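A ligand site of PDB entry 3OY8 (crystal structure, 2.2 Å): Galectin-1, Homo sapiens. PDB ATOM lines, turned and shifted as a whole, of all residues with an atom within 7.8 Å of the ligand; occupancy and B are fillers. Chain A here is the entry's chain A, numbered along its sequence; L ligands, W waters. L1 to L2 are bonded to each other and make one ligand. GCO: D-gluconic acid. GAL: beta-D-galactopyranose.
The side-chain carboxylate of Glu 71 sits at hydrogen-bond distance from an oxygen (O3) of GCO L1, 2.6 Å away.
The guanidinium group of Arg 48 lies within hydrogen-bond range of an oxygen (O3) of GCO L1 (2.7 Å).
An oxygen (O4) of GAL L2 sits at hydrogen-bond distance from a ring nitrogen (NE2) of His 44, at 2.8 Å.
The side-chain amide nitrogen (ND2) of Asn 61 lies within hydrogen-bond range of an oxygen (O6) of GAL L2, at 2.9 Å.
A ring nitrogen (NE2) of His 52 lies within hydrogen-bond range of an oxygen (O2) of GAL L2.
An oxygen (O4) of GAL L2 sits at hydrogen-bond distance from the side-chain amide oxygen of Asn 46 (3.4 Å).
The guanidinium group of Arg 73 lies within salt-bridge range of an oxygen (O1A) of GCO L1, 3.4 Å away.
The side-chain carboxylate (OE1) of Glu 71 is in salt-bridge range of the guanidinium group (NH1) of Arg 73 (2.4 Å).
The guanidinium group (NE) of Arg 48 lies within hydrogen-bond range of the side-chain amide oxygen (OD1) of Asn 46, 2.8 Å away.
The guanidinium group (NH1) of Arg 48 is in salt-bridge range of the side-chain carboxylate (OD2) of Asp 54 (2.8 Å).
A ring nitrogen (ND1) of His 44 lies within hydrogen-bond range of the side-chain amide oxygen (OD1) of Asn 33, 2.7 Å away.
The side-chain amide nitrogen of Asn 61 lies within hydrogen-bond range of the backbone carbonyl oxygen of Gly 69 (3.0 Å).
The backbone carbonyl oxygen (O) of Thr 70 sits close to the side-chain amide oxygen (OD1) of Asn 61, 3.3 Å away.
O of Val 59 sits at hydrogen-bond distance from N of Asn 46.
The side-chain amide nitrogen (ND2) of Asn 46 sits at hydrogen-bond distance from the side-chain hydroxyl (OG) of Ser 29 (3.0 Å).
CZ2 of Trp 68 touches C4 of GAL L2 (3.9 Å).
Hydrophobic or aromatic side chains within 4 Å of the ligand: His 44, His 52 and Trp 68.
The nearest printed residue that does not touch the ligand is Val 59 (4.5 Å).
Water W2 lies within hydrogen-bond range of O3 of GAL L2 (3.1 Å) and OD1 of Asn 46 (3.1 Å).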
ATOM      1  N   SER A  29      37.651 -35.450 -31.539  1.00  0.00           N
ATOM      2  CA  SER A  29      36.539 -34.541 -31.755  1.00  0.00           C
ATOM      3  C   SER A  29      36.534 -34.070 -33.209  1.00  0.00           C
ATOM      4  O   SER A  29      37.605 -33.948 -33.813  1.00  0.00           O
ATOM      5  CB  SER A  29      36.696 -33.326 -30.830  1.00  0.00           C
ATOM      6  OG  SER A  29      35.823 -32.271 -31.201  1.00  0.00           O
ATOM      7  N   PHE A  30      35.352 -33.809 -33.767  1.00  0.00           N
ATOM      8  CA  PHE A  30      35.249 -32.997 -34.989  1.00  0.00           C
ATOM      9  C   PHE A  30      34.035 -32.065 -34.979  1.00  0.00           C
ATOM     10  O   PHE A  30      33.089 -32.256 -34.204  1.00  0.00           O
ATOM     11  CB  PHE A  30      35.397 -33.827 -36.283  1.00  0.00           C
ATOM     12  CG  PHE A  30      34.128 -34.534 -36.749  1.00  0.00           C
ATOM     13  CD1 PHE A  30      33.229 -33.899 -37.596  1.00  0.00           C
ATOM     14  CD2 PHE A  30      33.888 -35.857 -36.375  1.00  0.00           C
ATOM     15  CE1 PHE A  30      32.074 -34.551 -38.055  1.00  0.00           C
ATOM     16  CE2 PHE A  30      32.741 -36.519 -36.822  1.00  0.00           C
ATOM     17  CZ  PHE A  30      31.834 -35.877 -37.659  1.00  0.00           C
ATOM     18  N   VAL A  31      34.092 -31.041 -35.822  1.00  0.00           N
ATOM     19  CA  VAL A  31      33.081 -29.996 -35.855  1.00  0.00           C
ATOM     20  C   VAL A  31      32.583 -29.747 -37.276  1.00  0.00           C
ATOM     21  O   VAL A  31      33.378 -29.669 -38.216  1.00  0.00           O
ATOM     22  CB  VAL A  31      33.635 -28.676 -35.242  1.00  0.00           C
ATOM     23  CG1 VAL A  31      32.668 -27.533 -35.443  1.00  0.00           C
ATOM     24  CG2 VAL A  31      33.925 -28.853 -33.751  1.00  0.00           C
ATOM     25  N   ASN A  33      30.190 -26.656 -38.711  1.00  0.00           N
ATOM     26  CA  ASN A  33      29.479 -25.421 -38.418  1.00  0.00           C
ATOM     27  C   ASN A  33      28.714 -24.958 -39.656  1.00  0.00           C
ATOM     28  O   ASN A  33      29.273 -24.902 -40.749  1.00  0.00           O
ATOM     29  CB  ASN A  33      30.456 -24.322 -37.968  1.00  0.00           C
ATOM     30  CG  ASN A  33      30.983 -24.529 -36.553  1.00  0.00           C
ATOM     31  OD1 ASN A  33      30.322 -25.135 -35.703  1.00  0.00           O
ATOM     32  ND2 ASN A  33      32.178 -24.030 -36.291  1.00  0.00           N
ATOM     33  N   HIS A  44      25.936 -25.876 -34.792  1.00  0.00           N
ATOM     34  CA  HIS A  44      27.271 -26.311 -34.415  1.00  0.00           C
ATOM     35  C   HIS A  44      27.123 -27.785 -34.046  1.00  0.00           C
ATOM     36  O   HIS A  44      26.518 -28.126 -33.040  1.00  0.00           O
ATOM     37  CB  HIS A  44      27.769 -25.477 -33.221  1.00  0.00           C
ATOM     38  CG  HIS A  44      29.004 -26.014 -32.578  1.00  0.00           C
ATOM     39  ND1 HIS A  44      30.265 -25.795 -33.097  1.00  0.00           N
ATOM     40  CD2 HIS A  44      29.177 -26.715 -31.434  1.00  0.00           C
ATOM     41  CE1 HIS A  44      31.164 -26.367 -32.310  1.00  0.00           C
ATOM     42  NE2 HIS A  44      30.533 -26.939 -31.303  1.00  0.00           N
ATOM     43  N   PHE A  45      27.652 -28.662 -34.911  1.00  0.00           N
ATOM     44  CA  PHE A  45      27.516 -30.119 -34.789  1.00  0.00           C
ATOM     45  C   PHE A  45      28.887 -30.663 -34.396  1.00  0.00           C
ATOM     46  O   PHE A  45      29.846 -30.566 -35.161  1.00  0.00           O
ATOM     47  CB  PHE A  45      27.055 -30.679 -36.140  1.00  0.00           C
ATOM     48  CG  PHE A  45      26.996 -32.193 -36.210  1.00  0.00           C
ATOM     49  CD1 PHE A  45      25.912 -32.891 -35.670  1.00  0.00           C
ATOM     50  CD2 PHE A  45      27.987 -32.912 -36.875  1.00  0.00           C
ATOM     51  CE1 PHE A  45      25.839 -34.290 -35.755  1.00  0.00           C
ATOM     52  CE2 PHE A  45      27.923 -34.305 -36.977  1.00  0.00           C
ATOM     53  CZ  PHE A  45      26.853 -34.995 -36.403  1.00  0.00           C
ATOM     54  N   ASN A  46      28.972 -31.222 -33.190  1.00  0.00           N
ATOM     55  CA  ASN A  46      30.270 -31.553 -32.584  1.00  0.00           C
ATOM     56  C   ASN A  46      30.272 -32.940 -31.919  1.00  0.00           C
ATOM     57  O   ASN A  46      30.079 -33.035 -30.697  1.00  0.00           O
ATOM     58  CB  ASN A  46      30.692 -30.422 -31.621  1.00  0.00           C
ATOM     59  CG  ASN A  46      32.009 -30.711 -30.862  1.00  0.00           C
ATOM     60  OD1 ASN A  46      32.173 -30.300 -29.716  1.00  0.00           O
ATOM     61  ND2 ASN A  46      32.949 -31.385 -31.514  1.00  0.00           N
ATOM     62  N   ARG A  48      31.835 -35.740 -30.048  1.00  0.00           N
ATOM     63  CA  ARG A  48      32.988 -35.868 -29.165  1.00  0.00           C
ATOM     64  C   ARG A  48      33.280 -37.335 -28.907  1.00  0.00           C
ATOM     65  O   ARG A  48      32.517 -38.016 -28.218  1.00  0.00           O
ATOM     66  CB  ARG A  48      32.755 -35.098 -27.865  1.00  0.00           C
ATOM     67  CG  ARG A  48      32.758 -33.584 -28.060  1.00  0.00           C
ATOM     68  CD  ARG A  48      32.240 -32.842 -26.847  1.00  0.00           C
ATOM     69  NE  ARG A  48      32.125 -31.403 -27.117  1.00  0.00           N
ATOM     70  CZ  ARG A  48      31.738 -30.487 -26.225  1.00  0.00           C
ATOM     71  NH1 ARG A  48      31.434 -30.843 -24.985  1.00  0.00           N
ATOM     72  NH2 ARG A  48      31.667 -29.212 -26.575  1.00  0.00           N
ATOM     73  N   ALA A  51      36.558 -35.702 -25.643  1.00  0.00           N
ATOM     74  CA  ALA A  51      36.865 -34.289 -25.479  1.00  0.00           C
ATOM     75  C   ALA A  51      35.930 -33.638 -24.467  1.00  0.00           C
ATOM     76  O   ALA A  51      34.750 -34.018 -24.373  1.00  0.00           O
ATOM     77  CB  ALA A  51      36.778 -33.568 -26.818  1.00  0.00           C
ATOM     78  N   HIS A  52      36.450 -32.661 -23.719  1.00  0.00           N
ATOM     79  CA  HIS A  52      35.702 -31.900 -22.701  1.00  0.00           C
ATOM     80  C   HIS A  52      35.037 -32.782 -21.631  1.00  0.00           C
ATOM     81  O   HIS A  52      33.986 -32.420 -21.084  1.00  0.00           O
ATOM     82  CB  HIS A  52      34.656 -30.985 -23.352  1.00  0.00           C
ATOM     83  CG  HIS A  52      35.245 -29.970 -24.298  1.00  0.00           C
ATOM     84  ND1 HIS A  52      35.369 -30.212 -25.649  1.00  0.00           N
ATOM     85  CD2 HIS A  52      35.733 -28.723 -24.087  1.00  0.00           C
ATOM     86  CE1 HIS A  52      35.910 -29.152 -26.228  1.00  0.00           C
ATOM     87  NE2 HIS A  52      36.136 -28.235 -25.300  1.00  0.00           N
ATOM     88  N   GLY A  53      35.648 -33.915 -21.327  1.00  0.00           N
ATOM     89  CA  GLY A  53      35.077 -34.855 -20.358  1.00  0.00           C
ATOM     90  C   GLY A  53      34.021 -35.784 -20.931  1.00  0.00           C
ATOM     91  O   GLY A  53      33.602 -36.736 -20.275  1.00  0.00           O
ATOM     92  N   ASP A  54      33.592 -35.496 -22.161  1.00  0.00           N
ATOM     93  CA  ASP A  54      32.576 -36.305 -22.862  1.00  0.00           C
ATOM     94  C   ASP A  54      33.182 -37.488 -23.615  1.00  0.00           C
ATOM     95  O   ASP A  54      34.317 -37.423 -24.088  1.00  0.00           O
ATOM     96  CB  ASP A  54      31.778 -35.445 -23.838  1.00  0.00           C
ATOM     97  CG  ASP A  54      30.963 -34.378 -23.150  1.00  0.00           C
ATOM     98  OD1 ASP A  54      30.164 -34.715 -22.256  1.00  0.00           O
ATOM     99  OD2 ASP A  54      31.103 -33.191 -23.528  1.00  0.00           O
ATOM    100  N   VAL A  59      27.284 -33.367 -29.409  1.00  0.00           N
ATOM    101  CA  VAL A  59      26.880 -32.105 -28.806  1.00  0.00           C
ATOM    102  C   VAL A  59      26.484 -31.157 -29.934  1.00  0.00           C
ATOM    103  O   VAL A  59      27.206 -30.997 -30.918  1.00  0.00           O
ATOM    104  CB  VAL A  59      28.050 -31.496 -27.978  1.00  0.00           C
ATOM    105  CG1 VAL A  59      27.672 -30.123 -27.417  1.00  0.00           C
ATOM    106  CG2 VAL A  59      28.451 -32.442 -26.859  1.00  0.00           C
ATOM    107  N   CYS A  60      25.307 -30.556 -29.795  1.00  0.00           N
ATOM    108  CA  CYS A  60      24.832 -29.559 -30.745  1.00  0.00           C
ATOM    109  C   CYS A  60      24.557 -28.259 -30.015  1.00  0.00           C
ATOM    110  O   CYS A  60      24.204 -28.259 -28.831  1.00  0.00           O
ATOM    111  CB  CYS A  60      23.555 -30.024 -31.438  1.00  0.00           C
ATOM    112  SG  CYS A  60      23.738 -31.454 -32.532  1.00  0.00           S
ATOM    113  N   ASN A  61      24.738 -27.149 -30.717  1.00  0.00           N
ATOM    114  CA  ASN A  61      24.440 -25.822 -30.177  1.00  0.00           C
ATOM    115  C   ASN A  61      24.274 -24.841 -31.327  1.00  0.00           C
ATOM    116  O   ASN A  61      24.467 -25.190 -32.502  1.00  0.00           O
ATOM    117  CB  ASN A  61      25.551 -25.361 -29.219  1.00  0.00           C
ATOM    118  CG  ASN A  61      25.061 -24.321 -28.195  1.00  0.00           C
ATOM    119  OD1 ASN A  61      23.923 -23.851 -28.257  1.00  0.00           O
ATOM    120  ND2 ASN A  61      25.922 -23.976 -27.252  1.00  0.00           N
ATOM    121  N   SER A  62      23.882 -23.621 -30.991  1.00  0.00           N
ATOM    122  CA  SER A  62      23.823 -22.528 -31.941  1.00  0.00           C
ATOM    123  C   SER A  62      24.748 -21.422 -31.445  1.00  0.00           C
ATOM    124  O   SER A  62      25.251 -21.477 -30.320  1.00  0.00           O
ATOM    125  CB  SER A  62      22.384 -22.019 -32.087  1.00  0.00           C
ATOM    126  OG  SER A  62      21.836 -21.643 -30.839  1.00  0.00           O
ATOM    127  N   LYS A  63      25.001 -20.433 -32.292  1.00  0.00           N
ATOM    128  CA  LYS A  63      25.758 -19.255 -31.894  1.00  0.00           C
ATOM    129  C   LYS A  63      25.078 -18.050 -32.525  1.00  0.00           C
ATOM    130  O   LYS A  63      24.817 -18.022 -33.734  1.00  0.00           O
ATOM    131  CB  LYS A  63      27.229 -19.360 -32.321  1.00  0.00           C
ATOM    132  CG  LYS A  63      28.128 -18.242 -31.764  1.00  0.00           C
ATOM    133  CD  LYS A  63      29.503 -18.221 -32.411  1.00  0.00           C
ATOM    134  CE  LYS A  63      30.549 -18.833 -31.502  1.00  0.00           C
ATOM    135  NZ  LYS A  63      31.873 -18.915 -32.187  1.00  0.00           N
ATOM    136  N   TRP A  68      27.151 -18.338 -27.662  1.00  0.00           N
ATOM    137  CA  TRP A  68      26.662 -19.712 -27.648  1.00  0.00           C
ATOM    138  C   TRP A  68      25.275 -19.799 -27.018  1.00  0.00           C
ATOM    139  O   TRP A  68      24.997 -19.159 -25.999  1.00  0.00           O
ATOM    140  CB  TRP A  68      27.614 -20.607 -26.862  1.00  0.00           C
ATOM    141  CG  TRP A  68      28.920 -20.893 -27.509  1.00  0.00           C
ATOM    142  CD1 TRP A  68      30.154 -20.526 -27.049  1.00  0.00           C
ATOM    143  CD2 TRP A  68      29.143 -21.618 -28.727  1.00  0.00           C
ATOM    144  NE1 TRP A  68      31.127 -20.979 -27.914  1.00  0.00           N
ATOM    145  CE2 TRP A  68      30.537 -21.649 -28.946  1.00  0.00           C
ATOM    146  CE3 TRP A  68      28.295 -22.248 -29.655  1.00  0.00           C
ATOM    147  CZ2 TRP A  68      31.114 -22.285 -30.056  1.00  0.00           C
ATOM    148  CZ3 TRP A  68      28.862 -22.877 -30.768  1.00  0.00           C
ATOM    149  CH2 TRP A  68      30.261 -22.893 -30.943  1.00  0.00           C
ATOM    150  N   GLY A  69      24.401 -20.591 -27.627  1.00  0.00           N
ATOM    151  CA  GLY A  69      23.072 -20.823 -27.088  1.00  0.00           C
ATOM    152  C   GLY A  69      23.080 -21.973 -26.091  1.00  0.00           C
ATOM    153  O   GLY A  69      24.135 -22.324 -25.547  1.00  0.00           O
ATOM    154  N   THR A  70      21.916 -22.562 -25.873  1.00  0.00           N
ATOM    155  CA  THR A  70      21.760 -23.693 -24.965  1.00  0.00           C
ATOM    156  C   THR A  70      22.132 -25.001 -25.660  1.00  0.00           C
ATOM    157  O   THR A  70      21.512 -25.388 -26.657  1.00  0.00           O
ATOM    158  CB  THR A  70      20.313 -23.786 -24.452  1.00  0.00           C
ATOM    159  OG1 THR A  70      19.980 -22.584 -23.750  1.00  0.00           O
ATOM    160  CG2 THR A  70      20.137 -24.983 -23.507  1.00  0.00           C
ATOM    161  N   GLU A  71      23.161 -25.654 -25.128  1.00  0.00           N
ATOM    162  CA  GLU A  71      23.642 -26.936 -25.615  1.00  0.00           C
ATOM    163  C   GLU A  71      22.585 -28.031 -25.528  1.00  0.00           C
ATOM    164  O   GLU A  71      21.837 -28.102 -24.550  1.00  0.00           O
ATOM    165  CB  GLU A  71      24.823 -27.397 -24.785  1.00  0.00           C
ATOM    166  CG  GLU A  71      26.172 -27.038 -25.340  1.00  0.00           C
ATOM    167  CD  GLU A  71      27.292 -27.737 -24.588  1.00  0.00           C
ATOM    168  OE1 GLU A  71      26.979 -28.551 -23.700  1.00  0.00           O
ATOM    169  OE2 GLU A  71      28.473 -27.460 -24.870  1.00  0.00           O
ATOM    170  N   GLN A  72      22.524 -28.866 -26.566  1.00  0.00           N
ATOM    171  CA  GLN A  72      21.735 -30.111 -26.545  1.00  0.00           C
ATOM    172  C   GLN A  72      22.648 -31.280 -26.864  1.00  0.00           C
ATOM    173  O   GLN A  72      23.533 -31.178 -27.724  1.00  0.00           O
ATOM    174  CB  GLN A  72      20.595 -30.059 -27.566  1.00  0.00           C
ATOM    175  CG  GLN A  72      19.444 -29.150 -27.154  1.00  0.00           C
ATOM    176  CD  GLN A  72      18.244 -29.251 -28.082  1.00  0.00           C
ATOM    177  OE1 GLN A  72      17.301 -28.457 -27.966  1.00  0.00           O
ATOM    178  NE2 GLN A  72      18.255 -30.214 -28.997  1.00  0.00           N
ATOM    179  N   ARG A  73      22.430 -32.400 -26.173  1.00  0.00           N
ATOM    180  CA  ARG A  73      23.152 -33.643 -26.464  1.00  0.00           C
ATOM    181  C   ARG A  73      22.204 -34.699 -27.037  1.00  0.00           C
ATOM    182  O   ARG A  73      21.045 -34.812 -26.628  1.00  0.00           O
ATOM    183  CB  ARG A  73      23.863 -34.145 -25.220  1.00  0.00           C
ATOM    184  CG  ARG A  73      25.146 -33.404 -24.911  1.00  0.00           C
ATOM    185  CD  ARG A  73      25.489 -33.457 -23.432  1.00  0.00           C
ATOM    186  NE  ARG A  73      26.920 -33.264 -23.190  1.00  0.00           N
ATOM    187  CZ  ARG A  73      27.544 -32.089 -23.167  1.00  0.00           C
ATOM    188  NH1 ARG A  73      26.854 -30.966 -23.373  1.00  0.00           N
ATOM    189  NH2 ARG A  73      28.846 -32.028 -22.942  1.00  0.00           N
HETATM  190  C1  GCO L   1      29.828 -29.100 -20.893  1.00  0.00           C
HETATM  191  C2  GCO L   1      30.115 -27.745 -21.478  1.00  0.00           C
HETATM  192  C3  GCO L   1      31.097 -27.852 -22.655  1.00  0.00           C
HETATM  193  C4  GCO L   1      31.530 -26.482 -23.195  1.00  0.00           C
HETATM  194  C5  GCO L   1      32.380 -25.686 -22.185  1.00  0.00           C
HETATM  195  C6  GCO L   1      33.825 -26.172 -22.098  1.00  0.00           C
HETATM  196  O1A GCO L   1      28.644 -29.453 -20.780  1.00  0.00           O
HETATM  197  O1B GCO L   1      30.787 -29.835 -20.555  1.00  0.00           O
HETATM  198  O2  GCO L   1      28.890 -27.147 -21.919  1.00  0.00           O
HETATM  199  O3  GCO L   1      30.520 -28.641 -23.710  1.00  0.00           O
HETATM  200  O4  GCO L   1      32.225 -26.642 -24.445  1.00  0.00           O
HETATM  201  O5  GCO L   1      32.369 -24.296 -22.536  1.00  0.00           O
HETATM  202  O6  GCO L   1      34.546 -25.345 -21.180  1.00  0.00           O
HETATM  203  C1  GAL L   2      32.040 -25.911 -25.538  1.00  0.00           C
HETATM  204  C2  GAL L   2      33.262 -26.057 -26.450  1.00  0.00           C
HETATM  205  C3  GAL L   2      33.037 -25.297 -27.766  1.00  0.00           C
HETATM  206  C4  GAL L   2      31.716 -25.724 -28.398  1.00  0.00           C
HETATM  207  C5  GAL L   2      30.586 -25.504 -27.388  1.00  0.00           C
HETATM  208  C6  GAL L   2      29.220 -25.904 -27.951  1.00  0.00           C
HETATM  209  O2  GAL L   2      34.416 -25.558 -25.798  1.00  0.00           O
HETATM  210  O3  GAL L   2      34.113 -25.534 -28.657  1.00  0.00           O
HETATM  211  O4  GAL L   2      31.780 -27.087 -28.788  1.00  0.00           O
HETATM  212  O5  GAL L   2      30.842 -26.269 -26.223  1.00  0.00           O
HETATM  213  O6  GAL L   2      28.232 -25.697 -26.979  1.00  0.00           O
HETATM  214  O   HOH W   1      28.614 -23.565 -24.502  1.00  0.00           O
HETATM  215  O   HOH W   2      34.643 -28.409 -29.633  1.00  0.00           O
